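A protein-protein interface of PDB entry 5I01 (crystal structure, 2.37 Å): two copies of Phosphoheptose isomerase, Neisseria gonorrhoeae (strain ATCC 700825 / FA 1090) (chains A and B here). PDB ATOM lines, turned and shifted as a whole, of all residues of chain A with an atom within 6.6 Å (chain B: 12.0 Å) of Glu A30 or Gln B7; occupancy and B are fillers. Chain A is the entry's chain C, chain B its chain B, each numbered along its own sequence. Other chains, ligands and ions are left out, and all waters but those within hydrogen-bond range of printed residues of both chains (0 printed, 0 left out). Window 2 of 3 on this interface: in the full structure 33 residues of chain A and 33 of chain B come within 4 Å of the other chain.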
ATOM      1  N   GLU A  25      20.911  -7.358 -26.747  1.00  0.00           N
ATOM      2  CA  GLU A  25      22.349  -7.582 -26.471  1.00  0.00           C
ATOM      3  C   GLU A  25      23.293  -6.569 -27.152  1.00  0.00           C
ATOM      4  O   GLU A  25      24.310  -6.195 -26.574  1.00  0.00           O
ATOM      5  CB  GLU A  25      22.744  -9.024 -26.869  1.00  0.00           C
ATOM      6  CG  GLU A  25      24.246  -9.311 -26.975  1.00  0.00           C
ATOM      7  CD  GLU A  25      24.568 -10.786 -27.208  1.00  0.00           C
ATOM      8  OE1 GLU A  25      23.816 -11.450 -27.962  1.00  0.00           O
ATOM      9  OE2 GLU A  25      25.586 -11.270 -26.638  1.00  0.00           O
ATOM     10  N   ILE A  27      22.810  -3.395 -28.000  1.00  0.00           N
ATOM     11  CA  ILE A  27      22.704  -2.017 -27.534  1.00  0.00           C
ATOM     12  C   ILE A  27      22.818  -1.830 -26.026  1.00  0.00           C
ATOM     13  O   ILE A  27      23.152  -0.732 -25.594  1.00  0.00           O
ATOM     14  CB  ILE A  27      21.397  -1.341 -28.006  1.00  0.00           C
ATOM     15  CG1 ILE A  27      20.153  -2.038 -27.457  1.00  0.00           C
ATOM     16  CG2 ILE A  27      21.317  -1.300 -29.529  1.00  0.00           C
ATOM     17  CD1 ILE A  27      18.982  -1.091 -27.334  1.00  0.00           C
ATOM     18  N   LEU A  28      22.541  -2.872 -25.233  1.00  0.00           N
ATOM     19  CA  LEU A  28      22.423  -2.726 -23.776  1.00  0.00           C
ATOM     20  C   LEU A  28      23.685  -3.059 -22.963  1.00  0.00           C
ATOM     21  O   LEU A  28      23.672  -2.896 -21.747  1.00  0.00           O
ATOM     22  CB  LEU A  28      21.220  -3.533 -23.249  1.00  0.00           C
ATOM     23  CG  LEU A  28      19.821  -2.982 -23.566  1.00  0.00           C
ATOM     24  CD1 LEU A  28      18.727  -3.935 -23.108  1.00  0.00           C
ATOM     25  CD2 LEU A  28      19.617  -1.611 -22.941  1.00  0.00           C
ATOM     26  N   VAL A  29      24.769  -3.490 -23.607  1.00  0.00           N
ATOM     27  CA  VAL A  29      25.992  -3.848 -22.876  1.00  0.00           C
ATOM     28  C   VAL A  29      26.615  -2.632 -22.173  1.00  0.00           C
ATOM     29  O   VAL A  29      26.839  -2.679 -20.963  1.00  0.00           O
ATOM     30  CB  VAL A  29      27.024  -4.591 -23.765  1.00  0.00           C
ATOM     31  CG1 VAL A  29      28.368  -4.724 -23.070  1.00  0.00           C
ATOM     32  CG2 VAL A  29      26.518  -5.983 -24.120  1.00  0.00           C
ATOM     33  N   GLU A  30      26.876  -1.552 -22.908  1.00  0.00           N
ATOM     34  CA  GLU A  30      27.565  -0.383 -22.324  1.00  0.00           C
ATOM     35  C   GLU A  30      26.760   0.333 -21.220  1.00  0.00           C
ATOM     36  O   GLU A  30      27.301   0.548 -20.130  1.00  0.00           O
ATOM     37  CB  GLU A  30      28.033   0.605 -23.409  1.00  0.00           C
ATOM     38  CG  GLU A  30      29.142   0.078 -24.316  1.00  0.00           C
ATOM     39  CD  GLU A  30      30.536   0.119 -23.694  1.00  0.00           C
ATOM     40  OE1 GLU A  30      30.667   0.339 -22.466  1.00  0.00           O
ATOM     41  OE2 GLU A  30      31.514  -0.089 -24.448  1.00  0.00           O
ATOM     42  N   PRO A  31      25.481   0.705 -21.487  1.00  0.00           N
ATOM     43  CA  PRO A  31      24.592   1.218 -20.431  1.00  0.00           C
ATOM     44  C   PRO A  31      24.527   0.379 -19.139  1.00  0.00           C
ATOM     45  O   PRO A  31      24.550   0.952 -18.057  1.00  0.00           O
ATOM     46  CB  PRO A  31      23.219   1.226 -21.106  1.00  0.00           C
ATOM     47  CG  PRO A  31      23.489   1.384 -22.552  1.00  0.00           C
ATOM     48  CD  PRO A  31      24.890   0.919 -22.825  1.00  0.00           C
ATOM     49  N   THR A  32      24.428  -0.950 -19.257  1.00  0.00           N
ATOM     50  CA  THR A  32      24.388  -1.858 -18.080  1.00  0.00           C
ATOM     51  C   THR A  32      25.641  -1.763 -17.205  1.00  0.00           C
ATOM     52  O   THR A  32      25.553  -1.834 -15.980  1.00  0.00           O
ATOM     53  CB  THR A  32      24.197  -3.337 -18.503  1.00  0.00           C
ATOM     54  OG1 THR A  32      23.041  -3.447 -19.338  1.00  0.00           O
ATOM     55  CG2 THR A  32      24.013  -4.258 -17.289  1.00  0.00           C
ATOM     56  N   VAL A  33      26.797  -1.630 -17.853  1.00  0.00           N
ATOM     57  CA  VAL A  33      28.084  -1.398 -17.180  1.00  0.00           C
ATOM     58  C   VAL A  33      28.108  -0.037 -16.486  1.00  0.00           C
ATOM     59  O   VAL A  33      28.659   0.086 -15.387  1.00  0.00           O
ATOM     60  CB  VAL A  33      29.264  -1.538 -18.183  1.00  0.00           C
ATOM     61  CG1 VAL A  33      30.567  -0.951 -17.645  1.00  0.00           C
ATOM     62  CG2 VAL A  33      29.449  -3.002 -18.556  1.00  0.00           C
ATOM     63  N   GLN A  34      27.527   0.976 -17.127  1.00  0.00           N
ATOM     64  CA  GLN A  34      27.402   2.308 -16.513  1.00  0.00           C
ATOM     65  C   GLN A  34      26.455   2.295 -15.304  1.00  0.00           C
ATOM     66  O   GLN A  34      26.703   2.982 -14.309  1.00  0.00           O
ATOM     67  CB  GLN A  34      26.957   3.358 -17.553  1.00  0.00           C
ATOM     68  CG  GLN A  34      28.013   3.653 -18.616  1.00  0.00           C
ATOM     69  CD  GLN A  34      27.524   4.599 -19.702  1.00  0.00           C
ATOM     70  OE1 GLN A  34      26.480   4.371 -20.324  1.00  0.00           O
ATOM     71  NE2 GLN A  34      28.283   5.665 -19.944  1.00  0.00           N
ATOM     72  N   ALA A  35      25.381   1.514 -15.399  1.00  0.00           N
ATOM     73  CA  ALA A  35      24.440   1.350 -14.299  1.00  0.00           C
ATOM     74  C   ALA A  35      25.100   0.702 -13.084  1.00  0.00           C
ATOM     75  O   ALA A  35      24.934   1.181 -11.967  1.00  0.00           O
ATOM     76  CB  ALA A  35      23.235   0.533 -14.745  1.00  0.00           C
ATOM     77  N   GLU A  37      28.363   0.569 -12.445  1.00  0.00           N
ATOM     78  CA  GLU A  37      29.389   1.494 -11.975  1.00  0.00           C
ATOM     79  C   GLU A  37      28.787   2.585 -11.109  1.00  0.00           C
ATOM     80  O   GLU A  37      29.413   3.025 -10.148  1.00  0.00           O
ATOM     81  CB  GLU A  37      30.137   2.120 -13.154  1.00  0.00           C
ATOM     82  CG  GLU A  37      31.183   1.187 -13.740  1.00  0.00           C
ATOM     83  CD  GLU A  37      31.750   1.638 -15.082  1.00  0.00           C
ATOM     84  OE1 GLU A  37      31.067   2.378 -15.836  1.00  0.00           O
ATOM     85  OE2 GLU A  37      32.891   1.223 -15.384  1.00  0.00           O
ATOM     86  N   VAL A 164      21.231   6.950 -15.978  1.00  0.00           N
ATOM     87  CA  VAL A 164      21.514   5.896 -16.966  1.00  0.00           C
ATOM     88  C   VAL A 164      20.196   5.238 -17.395  1.00  0.00           C
ATOM     89  O   VAL A 164      19.423   4.797 -16.540  1.00  0.00           O
ATOM     90  CB  VAL A 164      22.458   4.809 -16.389  1.00  0.00           C
ATOM     91  CG1 VAL A 164      22.737   3.717 -17.424  1.00  0.00           C
ATOM     92  CG2 VAL A 164      23.768   5.408 -15.895  1.00  0.00           C
ATOM     93  N   LEU A 166      18.108   2.255 -19.311  1.00  0.00           N
ATOM     94  CA  LEU A 166      18.182   0.874 -19.787  1.00  0.00           C
ATOM     95  C   LEU A 166      16.865   0.586 -20.494  1.00  0.00           C
ATOM     96  O   LEU A 166      15.902   0.104 -19.883  1.00  0.00           O
ATOM     97  CB  LEU A 166      18.467  -0.108 -18.632  1.00  0.00           C
ATOM     98  CG  LEU A 166      19.789   0.095 -17.862  1.00  0.00           C
ATOM     99  CD1 LEU A 166      20.036  -1.011 -16.852  1.00  0.00           C
ATOM    100  CD2 LEU A 166      20.978   0.183 -18.805  1.00  0.00           C
ATOM    101  N   CYS A 190      28.073  -8.034 -11.986  1.00  0.00           N
ATOM    102  CA  CYS A 190      29.098  -7.002 -12.156  1.00  0.00           C
ATOM    103  C   CYS A 190      29.539  -6.444 -10.810  1.00  0.00           C
ATOM    104  O   CYS A 190      30.740  -6.355 -10.552  1.00  0.00           O
ATOM    105  CB  CYS A 190      28.619  -5.861 -13.044  1.00  0.00           C
ATOM    106  SG  CYS A 190      28.762  -6.241 -14.787  1.00  0.00           S
ATOM    107  N   THR B   5      36.951  -7.661 -18.583  1.00  0.00           N
ATOM    108  CA  THR B   5      36.259  -6.351 -18.400  1.00  0.00           C
ATOM    109  C   THR B   5      34.786  -6.545 -18.094  1.00  0.00           C
ATOM    110  O   THR B   5      34.207  -7.599 -18.377  1.00  0.00           O
ATOM    111  CB  THR B   5      36.353  -5.444 -19.648  1.00  0.00           C
ATOM    112  OG1 THR B   5      35.618  -6.028 -20.733  1.00  0.00           O
ATOM    113  CG2 THR B   5      37.814  -5.204 -20.070  1.00  0.00           C
ATOM    114  N   LEU B   6      34.189  -5.506 -17.522  1.00  0.00           N
ATOM    115  CA  LEU B   6      32.765  -5.488 -17.214  1.00  0.00           C
ATOM    116  C   LEU B   6      31.897  -5.610 -18.469  1.00  0.00           C
ATOM    117  O   LEU B   6      30.823  -6.227 -18.425  1.00  0.00           O
ATOM    118  CB  LEU B   6      32.396  -4.212 -16.436  1.00  0.00           C
ATOM    119  CG  LEU B   6      32.906  -4.079 -14.998  1.00  0.00           C
ATOM    120  CD1 LEU B   6      32.328  -2.827 -14.356  1.00  0.00           C
ATOM    121  CD2 LEU B   6      32.551  -5.310 -14.171  1.00  0.00           C
ATOM    122  N   GLN B   7      32.364  -5.039 -19.575  1.00  0.00           N
ATOM    123  CA  GLN B   7      31.654  -5.147 -20.849  1.00  0.00           C
ATOM    124  C   GLN B   7      31.501  -6.618 -21.279  1.00  0.00           C
ATOM    125  O   GLN B   7      30.397  -7.066 -21.580  1.00  0.00           O
ATOM    126  CB  GLN B   7      32.350  -4.325 -21.949  1.00  0.00           C
ATOM    127  CG  GLN B   7      32.108  -2.814 -21.881  1.00  0.00           C
ATOM    128  CD  GLN B   7      32.910  -2.093 -20.790  1.00  0.00           C
ATOM    129  OE1 GLN B   7      33.713  -2.707 -20.059  1.00  0.00           O
ATOM    130  NE2 GLN B   7      32.701  -0.777 -20.682  1.00  0.00           N
ATOM    131  N   GLU B   8      32.608  -7.357 -21.268  1.00  0.00           N
ATOM    132  CA  GLU B   8      32.627  -8.770 -21.655  1.00  0.00           C
ATOM    133  C   GLU B   8      31.790  -9.641 -20.720  1.00  0.00           C
ATOM    134  O   GLU B   8      31.156 -10.602 -21.165  1.00  0.00           O
ATOM    135  CB  GLU B   8      34.072  -9.299 -21.694  1.00  0.00           C
ATOM    136  CG  GLU B   8      34.957  -8.697 -22.792  1.00  0.00           C
ATOM    137  CD  GLU B   8      36.377  -9.274 -22.818  1.00  0.00           C
ATOM    138  OE1 GLU B   8      37.035  -9.354 -21.747  1.00  0.00           O
ATOM    139  OE2 GLU B   8      36.841  -9.639 -23.925  1.00  0.00           O
ATOM    140  N   ARG B   9      31.795  -9.302 -19.430  1.00  0.00           N
ATOM    141  CA  ARG B   9      30.979  -9.994 -18.430  1.00  0.00           C
ATOM    142  C   ARG B   9      29.487  -9.865 -18.723  1.00  0.00           C
ATOM    143  O   ARG B   9      28.785 -10.868 -18.752  1.00  0.00           O
ATOM    144  CB  ARG B   9      31.286  -9.457 -17.037  1.00  0.00           C
ATOM    145  CG  ARG B   9      30.483 -10.093 -15.910  1.00  0.00           C
ATOM    146  CD  ARG B   9      31.185  -9.942 -14.567  1.00  0.00           C
ATOM    147  NE  ARG B   9      32.325 -10.859 -14.462  1.00  0.00           N
ATOM    148  CZ  ARG B   9      32.682 -11.555 -13.382  1.00  0.00           C
ATOM    149  NH1 ARG B   9      31.996 -11.497 -12.239  1.00  0.00           N
ATOM    150  NH2 ARG B   9      33.749 -12.347 -13.451  1.00  0.00           N
ATOM    151  N   VAL B  10      29.014  -8.641 -18.960  1.00  0.00           N
ATOM    152  CA  VAL B  10      27.606  -8.411 -19.323  1.00  0.00           C
ATOM    153  C   VAL B  10      27.279  -9.102 -20.651  1.00  0.00           C
ATOM    154  O   VAL B  10      26.244  -9.755 -20.767  1.00  0.00           O
ATOM    155  CB  VAL B  10      27.247  -6.900 -19.433  1.00  0.00           C
ATOM    156  CG1 VAL B  10      25.824  -6.695 -19.951  1.00  0.00           C
ATOM    157  CG2 VAL B  10      27.407  -6.195 -18.093  1.00  0.00           C
ATOM    158  N   ALA B  11      28.154  -8.953 -21.646  1.00  0.00           N
ATOM    159  CA  ALA B  11      27.962  -9.610 -22.949  1.00  0.00           C
ATOM    160  C   ALA B  11      27.739 -11.124 -22.816  1.00  0.00           C
ATOM    161  O   ALA B  11      26.860 -11.693 -23.477  1.00  0.00           O
ATOM    162  CB  ALA B  11      29.148  -9.331 -23.872  1.00  0.00           C
ATOM    163  N   ALA B  12      28.535 -11.749 -21.943  1.00  0.00           N
ATOM    164  CA  ALA B  12      28.466 -13.184 -21.680  1.00  0.00           C
ATOM    165  C   ALA B  12      27.168 -13.616 -20.985  1.00  0.00           C
ATOM    166  O   ALA B  12      26.653 -14.700 -21.278  1.00  0.00           O
ATOM    167  CB  ALA B  12      29.681 -13.633 -20.881  1.00  0.00           C
ATOM    168  N   HIS B  13      26.641 -12.783 -20.082  1.00  0.00           N
ATOM    169  CA  HIS B  13      25.318 -13.030 -19.470  1.00  0.00           C
ATOM    170  C   HIS B  13      24.203 -13.107 -20.495  1.00  0.00           C
ATOM    171  O   HIS B  13      23.369 -13.999 -20.422  1.00  0.00           O
ATOM    172  CB  HIS B  13      24.963 -11.962 -18.441  1.00  0.00           C
ATOM    173  CG  HIS B  13      25.567 -12.195 -17.096  1.00  0.00           C
ATOM    174  ND1 HIS B  13      24.809 -12.309 -15.954  1.00  0.00           N
ATOM    175  CD2 HIS B  13      26.855 -12.346 -16.709  1.00  0.00           C
ATOM    176  CE1 HIS B  13      25.604 -12.511 -14.918  1.00  0.00           C
ATOM    177  NE2 HIS B  13      26.852 -12.530 -15.350  1.00  0.00           N
ATOM    178  N   PHE B  14      24.182 -12.152 -21.424  1.00  0.00           N
ATOM    179  CA  PHE B  14      23.231 -12.146 -22.547  1.00  0.00           C
ATOM    180  C   PHE B  14      23.345 -13.415 -23.401  1.00  0.00           C
ATOM    181  O   PHE B  14      22.343 -14.090 -23.673  1.00  0.00           O
ATOM    182  CB  PHE B  14      23.451 -10.916 -23.439  1.00  0.00           C
ATOM    183  CG  PHE B  14      22.681  -9.691 -23.019  1.00  0.00           C
ATOM    184  CD1 PHE B  14      21.351  -9.515 -23.418  1.00  0.00           C
ATOM    185  CD2 PHE B  14      23.292  -8.682 -22.269  1.00  0.00           C
ATOM    186  CE1 PHE B  14      20.644  -8.361 -23.064  1.00  0.00           C
ATOM    187  CE2 PHE B  14      22.592  -7.532 -21.908  1.00  0.00           C
ATOM    188  CZ  PHE B  14      21.269  -7.369 -22.310  1.00  0.00           C
ATOM    189  N   ALA B  15      24.568 -13.736 -23.814  1.00  0.00           N
ATOM    190  CA  ALA B  15      24.815 -14.919 -24.650  1.00  0.00           C
ATOM    191  C   ALA B  15      24.461 -16.228 -23.926  1.00  0.00           C
ATOM    192  O   ALA B  15      23.809 -17.108 -24.499  1.00  0.00           O
ATOM    193  CB  ALA B  15      26.257 -14.930 -25.144  1.00  0.00           C
ATOM    194  N   GLU B  16      24.855 -16.336 -22.659  1.00  0.00           N
ATOM    195  CA  GLU B  16      24.463 -17.480 -21.830  1.00  0.00           C
ATOM    196  C   GLU B  16      22.930 -17.622 -21.762  1.00  0.00           C
ATOM    197  O   GLU B  16      22.398 -18.722 -21.924  1.00  0.00           O
ATOM    198  CB  GLU B  16      25.081 -17.384 -20.426  1.00  0.00           C
ATOM    199  CG  GLU B  16      25.080 -18.688 -19.631  1.00  0.00           C
ATOM    200  CD  GLU B  16      25.803 -18.571 -18.294  1.00  0.00           C
ATOM    201  OE1 GLU B  16      25.337 -17.797 -17.434  1.00  0.00           O
ATOM    202  OE2 GLU B  16      26.830 -19.258 -18.090  1.00  0.00           O
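Of the 14 printed residues of chain A, 7 touch a printed residue of chain B. Printed residues of chain A that touch a printed residue of chain B: Glu A25, Leu A28, Val A29, Glu A30, Thr A32, Val A33 and Cys A190. Of the 12 printed residues of chain B, 6 touch a printed residue of chain A. Hydrophobic or aromatic side chains of chain B that line the printed part of chain A: Leu B6, Val B10 and Phe B14. Among the printed residues, 12 pairs touch across the chains.
Glu A30 touches one residue of chain B. Of chain A, only Val A29, Glu A30 and Val A33 come within 4 Å of Gln B7. Printed residues of chain B within 4 Å of Val A29: Gln B7. No residue of chain B comes within 4 Å of Pro A31. Val A33 touches just these residues of chain B: Leu B6 (3.5 Å), Gln B7 (3.7 Å) and Val B10 (3.8 Å). No residue of chain B comes within 4 Å of Gln A34. Of the printed residues of chain B, Cys A190 touches Leu B6 and Val B10. Printed residues of chain B within 4 Å of Leu A28: Phe B14. Of the printed residues of chain A, Leu B6 touches Val A33 (3.5 Å) and Cys A190 (3.95 Å). Thr B5 touches none of the printed residues of chain A.
The side-chain carboxylate (OE2) of Glu A25 lies close to the backbone carbonyl oxygen (O) of Ala B11, at 3.4 Å. The side-chain carboxylate of Glu A30 sits at hydrogen-bond distance from the side-chain amide nitrogen of Gln B7 (2.9 Å).
The backbone carbonyl oxygen of Leu A28 is in hydrogen-bond range of the side-chain hydroxyl of Thr A32.
No position is printed for both chains.
Among the printed residues, pairs that only touch across the chains: Val A29 with Gln B7 (3.4 Å), Val A33 with Leu B6 (3.5 Å), Cys A190 with Val B10 (3.6 Å), Val A33 with Gln B7 (3.7 Å), Glu A25 with Phe B14 (3.7 Å), Val A33 with Val B10 (3.8 Å), Glu A25 with Ala B15 (3.9 Å), Leu A28 with Phe B14 (3.9 Å), Cys A190 with Leu B6 (3.95 Å) and Thr A32 with Val B10 (3.99 Å).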
